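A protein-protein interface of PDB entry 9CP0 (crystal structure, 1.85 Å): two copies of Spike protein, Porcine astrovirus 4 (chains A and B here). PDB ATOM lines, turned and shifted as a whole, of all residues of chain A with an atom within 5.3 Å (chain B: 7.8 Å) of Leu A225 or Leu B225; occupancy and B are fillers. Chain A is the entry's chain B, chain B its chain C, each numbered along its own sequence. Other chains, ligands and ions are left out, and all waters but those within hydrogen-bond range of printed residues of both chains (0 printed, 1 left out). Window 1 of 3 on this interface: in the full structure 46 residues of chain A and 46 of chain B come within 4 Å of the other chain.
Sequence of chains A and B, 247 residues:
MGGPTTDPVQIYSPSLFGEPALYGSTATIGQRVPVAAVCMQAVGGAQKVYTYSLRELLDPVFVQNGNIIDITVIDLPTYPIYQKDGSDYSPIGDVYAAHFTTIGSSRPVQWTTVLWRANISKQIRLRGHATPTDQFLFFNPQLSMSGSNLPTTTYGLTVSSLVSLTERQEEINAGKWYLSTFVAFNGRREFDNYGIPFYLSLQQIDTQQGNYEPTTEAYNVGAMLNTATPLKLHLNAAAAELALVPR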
ATOM      1  N   ALA A  21       2.908 -34.577  25.815  1.00  0.00           N
ATOM      2  CA  ALA A  21       3.810 -34.089  24.788  1.00  0.00           C
ATOM      3  C   ALA A  21       5.184 -34.736  24.931  1.00  0.00           C
ATOM      4  O   ALA A  21       5.546 -35.288  25.979  1.00  0.00           O
ATOM      5  CB  ALA A  21       3.937 -32.568  24.852  1.00  0.00           C
ATOM      6  N   LEU A  22       5.952 -34.658  23.846  1.00  0.00           N
ATOM      7  CA  LEU A  22       7.311 -35.178  23.829  1.00  0.00           C
ATOM      8  C   LEU A  22       8.134 -34.613  24.982  1.00  0.00           C
ATOM      9  O   LEU A  22       8.146 -33.402  25.216  1.00  0.00           O
ATOM     10  CB  LEU A  22       7.974 -34.827  22.507  1.00  0.00           C
ATOM     11  CG  LEU A  22       8.747 -35.992  21.890  1.00  0.00           C
ATOM     12  CD1 LEU A  22       7.840 -37.198  21.770  1.00  0.00           C
ATOM     13  CD2 LEU A  22       9.339 -35.587  20.560  1.00  0.00           C
ATOM     14  N   PHE A 138      11.808 -31.221  30.138  1.00  0.00           N
ATOM     15  CA  PHE A 138      10.758 -30.684  29.287  1.00  0.00           C
ATOM     16  C   PHE A 138      11.003 -29.199  29.097  1.00  0.00           C
ATOM     17  O   PHE A 138      11.303 -28.486  30.061  1.00  0.00           O
ATOM     18  CB  PHE A 138       9.377 -30.920  29.903  1.00  0.00           C
ATOM     19  CG  PHE A 138       8.236 -30.468  29.036  1.00  0.00           C
ATOM     20  CD1 PHE A 138       8.138 -30.870  27.711  1.00  0.00           C
ATOM     21  CD2 PHE A 138       7.263 -29.619  29.543  1.00  0.00           C
ATOM     22  CE1 PHE A 138       7.088 -30.448  26.920  1.00  0.00           C
ATOM     23  CE2 PHE A 138       6.215 -29.184  28.747  1.00  0.00           C
ATOM     24  CZ  PHE A 138       6.126 -29.604  27.444  1.00  0.00           C
ATOM     25  N   PHE A 139      10.869 -28.740  27.855  1.00  0.00           N
ATOM     26  CA  PHE A 139      10.937 -27.317  27.535  1.00  0.00           C
ATOM     27  C   PHE A 139       9.515 -26.786  27.610  1.00  0.00           C
ATOM     28  O   PHE A 139       8.777 -26.793  26.623  1.00  0.00           O
ATOM     29  CB  PHE A 139      11.559 -27.094  26.164  1.00  0.00           C
ATOM     30  CG  PHE A 139      13.043 -27.273  26.134  1.00  0.00           C
ATOM     31  CD1 PHE A 139      13.877 -26.307  26.660  1.00  0.00           C
ATOM     32  CD2 PHE A 139      13.604 -28.418  25.589  1.00  0.00           C
ATOM     33  CE1 PHE A 139      15.249 -26.464  26.634  1.00  0.00           C
ATOM     34  CE2 PHE A 139      14.975 -28.587  25.559  1.00  0.00           C
ATOM     35  CZ  PHE A 139      15.801 -27.613  26.084  1.00  0.00           C
ATOM     36  N   PRO A 141       6.584 -24.431  27.389  1.00  0.00           N
ATOM     37  CA  PRO A 141       6.315 -23.130  26.766  1.00  0.00           C
ATOM     38  C   PRO A 141       5.681 -22.174  27.767  1.00  0.00           C
ATOM     39  O   PRO A 141       4.750 -22.536  28.490  1.00  0.00           O
ATOM     40  CB  PRO A 141       5.350 -23.477  25.626  1.00  0.00           C
ATOM     41  CG  PRO A 141       5.610 -24.932  25.346  1.00  0.00           C
ATOM     42  CD  PRO A 141       5.875 -25.521  26.696  1.00  0.00           C
ATOM     43  N   TYR A 155      10.682 -20.512  26.653  1.00  0.00           N
ATOM     44  CA  TYR A 155      10.719 -21.907  27.071  1.00  0.00           C
ATOM     45  C   TYR A 155      11.675 -22.046  28.246  1.00  0.00           C
ATOM     46  O   TYR A 155      12.847 -21.672  28.140  1.00  0.00           O
ATOM     47  CB  TYR A 155      11.143 -22.818  25.913  1.00  0.00           C
ATOM     48  CG  TYR A 155      10.240 -22.699  24.703  1.00  0.00           C
ATOM     49  CD1 TYR A 155       9.104 -23.487  24.579  1.00  0.00           C
ATOM     50  CD2 TYR A 155      10.510 -21.782  23.698  1.00  0.00           C
ATOM     51  CE1 TYR A 155       8.269 -23.372  23.477  1.00  0.00           C
ATOM     52  CE2 TYR A 155       9.684 -21.659  22.598  1.00  0.00           C
ATOM     53  CZ  TYR A 155       8.565 -22.455  22.494  1.00  0.00           C
ATOM     54  OH  TYR A 155       7.741 -22.334  21.389  1.00  0.00           O
ATOM     55  N   TYR A 219      11.954 -27.016  17.054  1.00  0.00           N
ATOM     56  CA  TYR A 219      10.613 -27.359  16.594  1.00  0.00           C
ATOM     57  C   TYR A 219      10.639 -28.632  15.756  1.00  0.00           C
ATOM     58  O   TYR A 219       9.775 -29.504  15.912  1.00  0.00           O
ATOM     59  CB  TYR A 219      10.021 -26.208  15.776  1.00  0.00           C
ATOM     60  CG  TYR A 219      10.072 -24.837  16.414  1.00  0.00           C
ATOM     61  CD1 TYR A 219      10.001 -24.675  17.791  1.00  0.00           C
ATOM     62  CD2 TYR A 219      10.175 -23.697  15.625  1.00  0.00           C
ATOM     63  CE1 TYR A 219      10.040 -23.412  18.362  1.00  0.00           C
ATOM     64  CE2 TYR A 219      10.212 -22.434  16.186  1.00  0.00           C
ATOM     65  CZ  TYR A 219      10.147 -22.295  17.556  1.00  0.00           C
ATOM     66  OH  TYR A 219      10.191 -21.039  18.119  1.00  0.00           O
ATOM     67  N   GLY A 222      11.232 -31.450  17.810  1.00  0.00           N
ATOM     68  CA  GLY A 222      10.151 -31.503  18.771  1.00  0.00           C
ATOM     69  C   GLY A 222      10.556 -31.216  20.201  1.00  0.00           C
ATOM     70  O   GLY A 222       9.804 -31.557  21.122  1.00  0.00           O
ATOM     71  N   ALA A 223      11.728 -30.614  20.411  1.00  0.00           N
ATOM     72  CA  ALA A 223      12.147 -30.263  21.761  1.00  0.00           C
ATOM     73  C   ALA A 223      11.303 -29.119  22.320  1.00  0.00           C
ATOM     74  O   ALA A 223      11.007 -29.096  23.517  1.00  0.00           O
ATOM     75  CB  ALA A 223      13.629 -29.891  21.771  1.00  0.00           C
ATOM     76  N   MET A 224      10.908 -28.159  21.484  1.00  0.00           N
ATOM     77  CA  MET A 224      10.024 -27.084  21.925  1.00  0.00           C
ATOM     78  C   MET A 224       8.750 -27.058  21.103  1.00  0.00           C
ATOM     79  O   MET A 224       8.792 -27.067  19.869  1.00  0.00           O
ATOM     80  CB  MET A 224      10.688 -25.707  21.879  1.00  0.00           C
ATOM     81  CG  MET A 224      11.849 -25.521  22.820  1.00  0.00           C
ATOM     82  SD  MET A 224      13.184 -24.529  22.142  1.00  0.00           S
ATOM     83  CE  MET A 224      13.931 -23.921  23.663  1.00  0.00           C
ATOM     84  N   LEU A 225       7.623 -27.019  21.795  1.00  0.00           N
ATOM     85  CA  LEU A 225       6.339 -27.020  21.126  1.00  0.00           C
ATOM     86  C   LEU A 225       6.071 -25.662  20.493  1.00  0.00           C
ATOM     87  O   LEU A 225       6.566 -24.623  20.941  1.00  0.00           O
ATOM     88  CB  LEU A 225       5.208 -27.360  22.095  1.00  0.00           C
ATOM     89  CG  LEU A 225       5.146 -28.766  22.679  1.00  0.00           C
ATOM     90  CD1 LEU A 225       6.182 -28.937  23.784  1.00  0.00           C
ATOM     91  CD2 LEU A 225       3.759 -29.057  23.200  1.00  0.00           C
ATOM     92  N   ASN A 226       5.293 -25.686  19.424  1.00  0.00           N
ATOM     93  CA  ASN A 226       4.821 -24.471  18.797  1.00  0.00           C
ATOM     94  C   ASN A 226       3.513 -24.797  18.104  1.00  0.00           C
ATOM     95  O   ASN A 226       3.067 -25.948  18.073  1.00  0.00           O
ATOM     96  CB  ASN A 226       5.852 -23.885  17.828  1.00  0.00           C
ATOM     97  CG  ASN A 226       5.830 -22.362  17.800  1.00  0.00           C
ATOM     98  OD1 ASN A 226       4.794 -21.736  18.040  1.00  0.00           O
ATOM     99  ND2 ASN A 226       6.978 -21.757  17.501  1.00  0.00           N
ATOM    100  N   THR A 227       2.896 -23.767  17.560  1.00  0.00           N
ATOM    101  CA  THR A 227       1.546 -23.900  17.042  1.00  0.00           C
ATOM    102  C   THR A 227       1.572 -24.464  15.627  1.00  0.00           C
ATOM    103  O   THR A 227       2.365 -24.024  14.787  1.00  0.00           O
ATOM    104  CB  THR A 227       0.842 -22.551  17.079  1.00  0.00           C
ATOM    105  OG1 THR A 227       0.575 -22.204  18.444  1.00  0.00           O
ATOM    106  CG2 THR A 227      -0.458 -22.608  16.309  1.00  0.00           C
ATOM    107  N   SER B  15       7.159 -23.124  11.969  1.00  0.00           N
ATOM    108  CA  SER B  15       7.133 -21.824  12.617  1.00  0.00           C
ATOM    109  C   SER B  15       8.407 -21.050  12.292  1.00  0.00           C
ATOM    110  O   SER B  15       9.445 -21.625  11.962  1.00  0.00           O
ATOM    111  CB  SER B  15       6.979 -21.985  14.130  1.00  0.00           C
ATOM    112  OG  SER B  15       5.710 -22.536  14.448  1.00  0.00           O
ATOM    113  N   GLU B  19       8.976 -17.422  16.627  1.00  0.00           N
ATOM    114  CA  GLU B  19       7.576 -17.068  16.441  1.00  0.00           C
ATOM    115  C   GLU B  19       6.755 -17.523  17.646  1.00  0.00           C
ATOM    116  O   GLU B  19       6.835 -18.695  18.037  1.00  0.00           O
ATOM    117  CB  GLU B  19       7.040 -17.703  15.156  1.00  0.00           C
ATOM    118  CG  GLU B  19       5.519 -17.857  15.094  1.00  0.00           C
ATOM    119  CD  GLU B  19       4.974 -17.700  13.678  1.00  0.00           C
ATOM    120  OE1 GLU B  19       5.342 -18.509  12.804  1.00  0.00           O
ATOM    121  OE2 GLU B  19       4.169 -16.773  13.448  1.00  0.00           O
ATOM    122  N   PRO B  20       5.981 -16.630  18.270  1.00  0.00           N
ATOM    123  CA  PRO B  20       5.167 -17.029  19.424  1.00  0.00           C
ATOM    124  C   PRO B  20       4.119 -18.069  19.066  1.00  0.00           C
ATOM    125  O   PRO B  20       3.648 -18.150  17.930  1.00  0.00           O
ATOM    126  CB  PRO B  20       4.503 -15.710  19.851  1.00  0.00           C
ATOM    127  CG  PRO B  20       5.442 -14.659  19.377  1.00  0.00           C
ATOM    128  CD  PRO B  20       5.934 -15.175  18.051  1.00  0.00           C
ATOM    129  N   ALA B  21       3.739 -18.861  20.065  1.00  0.00           N
ATOM    130  CA  ALA B  21       2.623 -19.783  19.930  1.00  0.00           C
ATOM    131  C   ALA B  21       1.297 -19.047  20.055  1.00  0.00           C
ATOM    132  O   ALA B  21       1.210 -17.957  20.633  1.00  0.00           O
ATOM    133  CB  ALA B  21       2.696 -20.882  20.988  1.00  0.00           C
ATOM    134  N   LEU B  22       0.256 -19.661  19.487  1.00  0.00           N
ATOM    135  CA  LEU B  22      -1.093 -19.122  19.591  1.00  0.00           C
ATOM    136  C   LEU B  22      -1.441 -18.781  21.034  1.00  0.00           C
ATOM    137  O   LEU B  22      -1.095 -19.508  21.970  1.00  0.00           O
ATOM    138  CB  LEU B  22      -2.111 -20.131  19.068  1.00  0.00           C
ATOM    139  CG  LEU B  22      -2.675 -19.980  17.654  1.00  0.00           C
ATOM    140  CD1 LEU B  22      -4.014 -20.668  17.652  1.00  0.00           C
ATOM    141  CD2 LEU B  22      -2.792 -18.516  17.243  1.00  0.00           C
ATOM    142  N   ARG B  55      -0.802 -14.215  14.012  1.00  0.00           N
ATOM    143  CA  ARG B  55       0.281 -15.186  13.892  1.00  0.00           C
ATOM    144  C   ARG B  55       0.474 -15.599  12.441  1.00  0.00           C
ATOM    145  O   ARG B  55      -0.381 -16.282  11.867  1.00  0.00           O
ATOM    146  CB  ARG B  55       0.032 -16.434  14.740  1.00  0.00           C
ATOM    147  CG  ARG B  55       1.261 -17.342  14.787  1.00  0.00           C
ATOM    148  CD  ARG B  55       1.042 -18.589  15.629  1.00  0.00           C
ATOM    149  NE  ARG B  55       2.265 -19.368  15.806  1.00  0.00           N
ATOM    150  CZ  ARG B  55       2.740 -20.280  14.964  1.00  0.00           C
ATOM    151  NH1 ARG B  55       2.127 -20.562  13.828  1.00  0.00           N
ATOM    152  NH2 ARG B  55       3.860 -20.926  15.277  1.00  0.00           N
ATOM    153  N   PHE B 138      -3.052 -17.886  28.048  1.00  0.00           N
ATOM    154  CA  PHE B 138      -2.259 -18.953  27.454  1.00  0.00           C
ATOM    155  C   PHE B 138      -2.360 -20.186  28.334  1.00  0.00           C
ATOM    156  O   PHE B 138      -2.296 -20.079  29.563  1.00  0.00           O
ATOM    157  CB  PHE B 138      -0.798 -18.513  27.284  1.00  0.00           C
ATOM    158  CG  PHE B 138       0.071 -19.517  26.560  1.00  0.00           C
ATOM    159  CD1 PHE B 138      -0.126 -19.804  25.221  1.00  0.00           C
ATOM    160  CD2 PHE B 138       1.109 -20.147  27.225  1.00  0.00           C
ATOM    161  CE1 PHE B 138       0.684 -20.721  24.566  1.00  0.00           C
ATOM    162  CE2 PHE B 138       1.917 -21.066  26.577  1.00  0.00           C
ATOM    163  CZ  PHE B 138       1.705 -21.344  25.245  1.00  0.00           C
ATOM    164  N   PHE B 139      -2.524 -21.350  27.704  1.00  0.00           N
ATOM    165  CA  PHE B 139      -2.502 -22.626  28.415  1.00  0.00           C
ATOM    166  C   PHE B 139      -1.093 -23.183  28.316  1.00  0.00           C
ATOM    167  O   PHE B 139      -0.734 -23.820  27.325  1.00  0.00           O
ATOM    168  CB  PHE B 139      -3.522 -23.602  27.840  1.00  0.00           C
ATOM    169  CG  PHE B 139      -4.945 -23.206  28.073  1.00  0.00           C
ATOM    170  CD1 PHE B 139      -5.554 -23.477  29.282  1.00  0.00           C
ATOM    171  CD2 PHE B 139      -5.685 -22.591  27.072  1.00  0.00           C
ATOM    172  CE1 PHE B 139      -6.871 -23.129  29.505  1.00  0.00           C
ATOM    173  CE2 PHE B 139      -7.001 -22.247  27.284  1.00  0.00           C
ATOM    174  CZ  PHE B 139      -7.596 -22.512  28.500  1.00  0.00           C
ATOM    175  N   ASN B 140      -0.299 -22.968  29.355  1.00  0.00           N
ATOM    176  CA  ASN B 140       1.114 -23.315  29.294  1.00  0.00           C
ATOM    177  C   ASN B 140       1.310 -24.798  29.585  1.00  0.00           C
ATOM    178  O   ASN B 140       1.009 -25.246  30.697  1.00  0.00           O
ATOM    179  CB  ASN B 140       1.907 -22.451  30.266  1.00  0.00           C
ATOM    180  CG  ASN B 140       1.362 -22.506  31.679  1.00  0.00           C
ATOM    181  OD1 ASN B 140       0.267 -22.019  31.955  1.00  0.00           O
ATOM    182  ND2 ASN B 140       2.144 -23.070  32.592  1.00  0.00           N
ATOM    183  N   PRO B 141       1.783 -25.592  28.622  1.00  0.00           N
ATOM    184  CA  PRO B 141       2.027 -27.014  28.895  1.00  0.00           C
ATOM    185  C   PRO B 141       3.042 -27.182  30.012  1.00  0.00           C
ATOM    186  O   PRO B 141       4.121 -26.585  29.992  1.00  0.00           O
ATOM    187  CB  PRO B 141       2.567 -27.555  27.564  1.00  0.00           C
ATOM    188  CG  PRO B 141       2.173 -26.548  26.532  1.00  0.00           C
ATOM    189  CD  PRO B 141       2.104 -25.219  27.236  1.00  0.00           C
ATOM    190  N   THR B 153       1.722 -34.405  30.633  1.00  0.00           N
ATOM    191  CA  THR B 153       1.648 -32.980  30.313  1.00  0.00           C
ATOM    192  C   THR B 153       0.328 -32.420  30.839  1.00  0.00           C
ATOM    193  O   THR B 153      -0.743 -32.802  30.357  1.00  0.00           O
ATOM    194  CB  THR B 153       1.749 -32.734  28.806  1.00  0.00           C
ATOM    195  OG1 THR B 153       2.738 -33.593  28.234  1.00  0.00           O
ATOM    196  CG2 THR B 153       2.160 -31.295  28.545  1.00  0.00           C
ATOM    197  N   THR B 154       0.400 -31.506  31.809  1.00  0.00           N
ATOM    198  CA  THR B 154      -0.751 -30.728  32.251  1.00  0.00           C
ATOM    199  C   THR B 154      -0.683 -29.326  31.664  1.00  0.00           C
ATOM    200  O   THR B 154       0.375 -28.860  31.234  1.00  0.00           O
ATOM    201  CB  THR B 154      -0.819 -30.607  33.777  1.00  0.00           C
ATOM    202  OG1 THR B 154       0.427 -30.103  34.267  1.00  0.00           O
ATOM    203  CG2 THR B 154      -1.126 -31.945  34.428  1.00  0.00           C
ATOM    204  N   TYR B 155      -1.818 -28.632  31.708  1.00  0.00           N
ATOM    205  CA  TYR B 155      -1.929 -27.288  31.160  1.00  0.00           C
ATOM    206  C   TYR B 155      -2.496 -26.363  32.223  1.00  0.00           C
ATOM    207  O   TYR B 155      -3.561 -26.635  32.785  1.00  0.00           O
ATOM    208  CB  TYR B 155      -2.803 -27.274  29.906  1.00  0.00           C
ATOM    209  CG  TYR B 155      -2.267 -28.140  28.788  1.00  0.00           C
ATOM    210  CD1 TYR B 155      -1.362 -27.634  27.867  1.00  0.00           C
ATOM    211  CD2 TYR B 155      -2.655 -29.469  28.660  1.00  0.00           C
ATOM    212  CE1 TYR B 155      -0.863 -28.418  26.848  1.00  0.00           C
ATOM    213  CE2 TYR B 155      -2.163 -30.261  27.634  1.00  0.00           C
ATOM    214  CZ  TYR B 155      -1.267 -29.728  26.733  1.00  0.00           C
ATOM    215  OH  TYR B 155      -0.768 -30.512  25.719  1.00  0.00           O
ATOM    216  N   PRO B 214      -7.229 -31.519  29.532  1.00  0.00           N
ATOM    217  CA  PRO B 214      -7.129 -31.385  28.076  1.00  0.00           C
ATOM    218  C   PRO B 214      -8.332 -31.964  27.358  1.00  0.00           C
ATOM    219  O   PRO B 214      -8.965 -32.921  27.809  1.00  0.00           O
ATOM    220  CB  PRO B 214      -5.851 -32.165  27.735  1.00  0.00           C
ATOM    221  CG  PRO B 214      -5.601 -33.083  28.917  1.00  0.00           C
ATOM    222  CD  PRO B 214      -6.599 -32.759  30.011  1.00  0.00           C
ATOM    223  N   ALA B 218      -9.541 -28.735  22.013  1.00  0.00           N
ATOM    224  CA  ALA B 218      -8.550 -27.708  22.321  1.00  0.00           C
ATOM    225  C   ALA B 218      -7.275 -27.908  21.514  1.00  0.00           C
ATOM    226  O   ALA B 218      -6.584 -26.932  21.192  1.00  0.00           O
ATOM    227  CB  ALA B 218      -8.239 -27.703  23.819  1.00  0.00           C
ATOM    228  N   TYR B 219      -6.931 -29.162  21.203  1.00  0.00           N
ATOM    229  CA  TYR B 219      -5.854 -29.425  20.257  1.00  0.00           C
ATOM    230  C   TYR B 219      -6.223 -28.924  18.868  1.00  0.00           C
ATOM    231  O   TYR B 219      -5.402 -28.305  18.182  1.00  0.00           O
ATOM    232  CB  TYR B 219      -5.550 -30.923  20.200  1.00  0.00           C
ATOM    233  CG  TYR B 219      -5.117 -31.580  21.491  1.00  0.00           C
ATOM    234  CD1 TYR B 219      -4.408 -30.885  22.459  1.00  0.00           C
ATOM    235  CD2 TYR B 219      -5.426 -32.911  21.737  1.00  0.00           C
ATOM    236  CE1 TYR B 219      -4.011 -31.507  23.640  1.00  0.00           C
ATOM    237  CE2 TYR B 219      -5.038 -33.537  22.901  1.00  0.00           C
ATOM    238  CZ  TYR B 219      -4.334 -32.833  23.853  1.00  0.00           C
ATOM    239  OH  TYR B 219      -3.955 -33.466  25.015  1.00  0.00           O
ATOM    240  N   GLY B 222      -6.041 -25.223  18.551  1.00  0.00           N
ATOM    241  CA  GLY B 222      -4.750 -24.670  18.890  1.00  0.00           C
ATOM    242  C   GLY B 222      -4.664 -24.048  20.266  1.00  0.00           C
ATOM    243  O   GLY B 222      -3.713 -23.310  20.539  1.00  0.00           O
ATOM    244  N   ALA B 223      -5.625 -24.321  21.148  1.00  0.00           N
ATOM    245  CA  ALA B 223      -5.593 -23.691  22.464  1.00  0.00           C
ATOM    246  C   ALA B 223      -4.558 -24.345  23.376  1.00  0.00           C
ATOM    247  O   ALA B 223      -3.911 -23.659  24.173  1.00  0.00           O
ATOM    248  CB  ALA B 223      -6.978 -23.733  23.110  1.00  0.00           C
ATOM    249  N   MET B 224      -4.385 -25.662  23.277  1.00  0.00           N
ATOM    250  CA  MET B 224      -3.338 -26.374  23.998  1.00  0.00           C
ATOM    251  C   MET B 224      -2.351 -26.979  23.013  1.00  0.00           C
ATOM    252  O   MET B 224      -2.748 -27.686  22.083  1.00  0.00           O
ATOM    253  CB  MET B 224      -3.912 -27.468  24.905  1.00  0.00           C
ATOM    254  CG  MET B 224      -4.619 -26.965  26.163  1.00  0.00           C
ATOM    255  SD  MET B 224      -5.939 -28.055  26.742  1.00  0.00           S
ATOM    256  CE  MET B 224      -6.980 -26.881  27.590  1.00  0.00           C
ATOM    257  N   LEU B 225      -1.070 -26.700  23.224  1.00  0.00           N
ATOM    258  CA  LEU B 225      -0.020 -27.232  22.372  1.00  0.00           C
ATOM    259  C   LEU B 225       0.155 -28.728  22.608  1.00  0.00           C
ATOM    260  O   LEU B 225      -0.014 -29.227  23.724  1.00  0.00           O
ATOM    261  CB  LEU B 225       1.296 -26.503  22.645  1.00  0.00           C
ATOM    262  CG  LEU B 225       1.310 -25.047  22.197  1.00  0.00           C
ATOM    263  CD1 LEU B 225       2.552 -24.336  22.714  1.00  0.00           C
ATOM    264  CD2 LEU B 225       1.254 -24.992  20.690  1.00  0.00           C
ATOM    265  N   ASN B 226       0.488 -29.448  21.543  1.00  0.00           N
ATOM    266  CA  ASN B 226       0.907 -30.834  21.690  1.00  0.00           C
ATOM    267  C   ASN B 226       1.890 -31.153  20.575  1.00  0.00           C
ATOM    268  O   ASN B 226       2.137 -30.344  19.679  1.00  0.00           O
ATOM    269  CB  ASN B 226      -0.287 -31.803  21.691  1.00  0.00           C
ATOM    270  CG  ASN B 226      -0.066 -33.008  22.611  1.00  0.00           C
ATOM    271  OD1 ASN B 226       1.064 -33.452  22.816  1.00  0.00           O
ATOM    272  ND2 ASN B 226      -1.151 -33.538  23.161  1.00  0.00           N
ATOM    273  N   THR B 227       2.463 -32.345  20.652  1.00  0.00           N
ATOM    274  CA  THR B 227       3.552 -32.730  19.769  1.00  0.00           C
ATOM    275  C   THR B 227       3.015 -33.100  18.386  1.00  0.00           C
ATOM    276  O   THR B 227       2.072 -33.892  18.263  1.00  0.00           O
ATOM    277  CB  THR B 227       4.327 -33.892  20.387  1.00  0.00           C
ATOM    278  OG1 THR B 227       4.998 -33.438  21.571  1.00  0.00           O
ATOM    279  CG2 THR B 227       5.352 -34.446  19.409  1.00  0.00           C
ATOM    280  N   ALA B 228       3.599 -32.493  17.353  1.00  0.00           N
ATOM    281  CA  ALA B 228       3.265 -32.794  15.961  1.00  0.00           C
ATOM    282  C   ALA B 228       1.764 -32.714  15.704  1.00  0.00           C
ATOM    283  O   ALA B 228       1.235 -33.387  14.815  1.00  0.00           O
ATOM    284  CB  ALA B 228       3.798 -34.169  15.556  1.00  0.00           C
ATOM    285  N   THR B 229       1.058 -31.892  16.478  1.00  0.00           N
ATOM    286  CA  THR B 229      -0.390 -31.855  16.377  1.00  0.00           C
ATOM    287  C   THR B 229      -0.813 -30.733  15.445  1.00  0.00           C
ATOM    288  O   THR B 229      -0.513 -29.566  15.725  1.00  0.00           O
ATOM    289  CB  THR B 229      -1.032 -31.664  17.736  1.00  0.00           C
ATOM    290  OG1 THR B 229      -0.662 -32.749  18.594  1.00  0.00           O
ATOM    291  CG2 THR B 229      -2.546 -31.644  17.586  1.00  0.00           C
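Ala A21 touches Asn B226, and with the chains exchanged Asn A226 touches Ala B21.
Ala A21 touches Thr B227, and with the chains exchanged Thr A227 touches Ala B21.
Leu B225 touches its own counterpart, Leu A225.
Thr A227 touches Leu B225, but with the chains exchanged Leu A225 does not touch Thr B227 (4.4 Å).
Positions printed for both chains: 21, 22, 138, 139, 141, 155, 219, 222, 223, 224, 225, 226 and 227.
Of the 22 pairs that touch across the chains among the printed residues, 12 have their exchanged pair printed and touching as well.
The backbone NH of Ala A21 sits at hydrogen-bond distance from the side-chain hydroxyl of Thr B153.
ND2 of Asn A226 lies close to OG of Ser B15 (3.4 Å).
O of Thr A227 is in hydrogen-bond range of NH2 of Arg B55 (3.5 Å).
ND2 of Asn A226 sits at hydrogen-bond distance from O of Glu B19 (3.1 Å).
N of Leu A22 sits at hydrogen-bond distance from OG1 of Thr B227, 2.8 Å away.
OD1 of Asn A226 lies within hydrogen-bond range of NH2 of Arg B55, at 3.0 Å.
N of Leu B22 lies within hydrogen-bond range of OG1 of Thr A227, at 2.8 Å.
Of the printed residues of chain A, Leu B225 touches Leu A225, Asn A226 and Thr A227.
Printed residues of chain B within 4 Å of Thr A227: Ser B15 (3.7 Å), Ala B21 (3.5 Å), Leu B22 (2.8 Å), Arg B55 (3.5 Å) and Leu B225 (3.6 Å).
Printed residues of chain B within 4 Å of Pro A141: Phe B138 (3.7 Å), Asn B140 (3.4 Å) and Pro B141 (3.8 Å).
Of the printed residues of chain A, Glu B19 touches Asn A226.
Of the printed residues of chain B, Tyr A219 touches Ser B15.
Of the printed residues of chain A, Thr B227 touches Ala A21 and Leu A22.
Pro B214 touches none of the printed residues of chain A.
Ala A223 touches none of the printed residues of chain B.
The nearest residue of chain B that does not touch Leu A225 is Thr B227 (4.4 Å).
The nearest residue of chain A that does not touch Leu B225 is Pro A141 (4.1 Å).
The nearest printed residue of chain A that does not touch Thr B153 is Phe A138 (4.4 Å).
OH of Tyr A155 is in hydrogen-bond range of O of Leu A225, 2.6 Å away.
OE1 of Glu B19 is in salt-bridge range of NH2 of Arg B55, at 3.8 Å.
OH of Tyr B155 lies within hydrogen-bond range of O of Leu B225 (2.5 Å).
The backbone carbonyl oxygen (O) of Thr B227 lies within hydrogen-bond range of the side-chain hydroxyl (OG1) of Thr B229, at 3.0 Å.
The side-chain hydroxyl (OG) of Ser B15 sits at hydrogen-bond distance from the guanidinium group (NH2) of Arg B55 (2.6 Å).
OH of Tyr A219 sits close to ND2 of Asn A226 (3.3 Å).
Of the 13 printed residues of chain A, 8 touch a printed residue of chain B.
Hydrophobic or aromatic side chains of chain A within 4 Å of the printed part of chain B: Ala A21, Leu A22, Phe A138, Pro A141, Tyr A219 and Leu A225.
Among the printed residues, 22 pairs touch across the chains.
Among the printed residues, merely in contact across the chains: Asn A226 with Leu B225 (3.3 Å), Pro A141 with Asn B140 (3.4 Å), Ala A21 with Asn B226 (3.4 Å), Asn A226 with Ala B21 (3.5 Å), Ala A21 with Thr B227 (3.5 Å), Thr A227 with Ala B21 (3.5 Å), Phe A138 with Pro B141 (3.6 Å), Leu A225 with Leu B225 (3.6 Å), Thr A227 with Leu B225 (3.6 Å), Thr A227 with Ser B15 (3.7 Å), Leu A225 with Asn B226 (3.7 Å), Pro A141 with Phe B138 (3.7 Å), Asn A226 with Pro B20 (3.8 Å), Pro A141 with Pro B141 (3.8 Å) and Tyr A219 with Ser B15 (3.9 Å).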
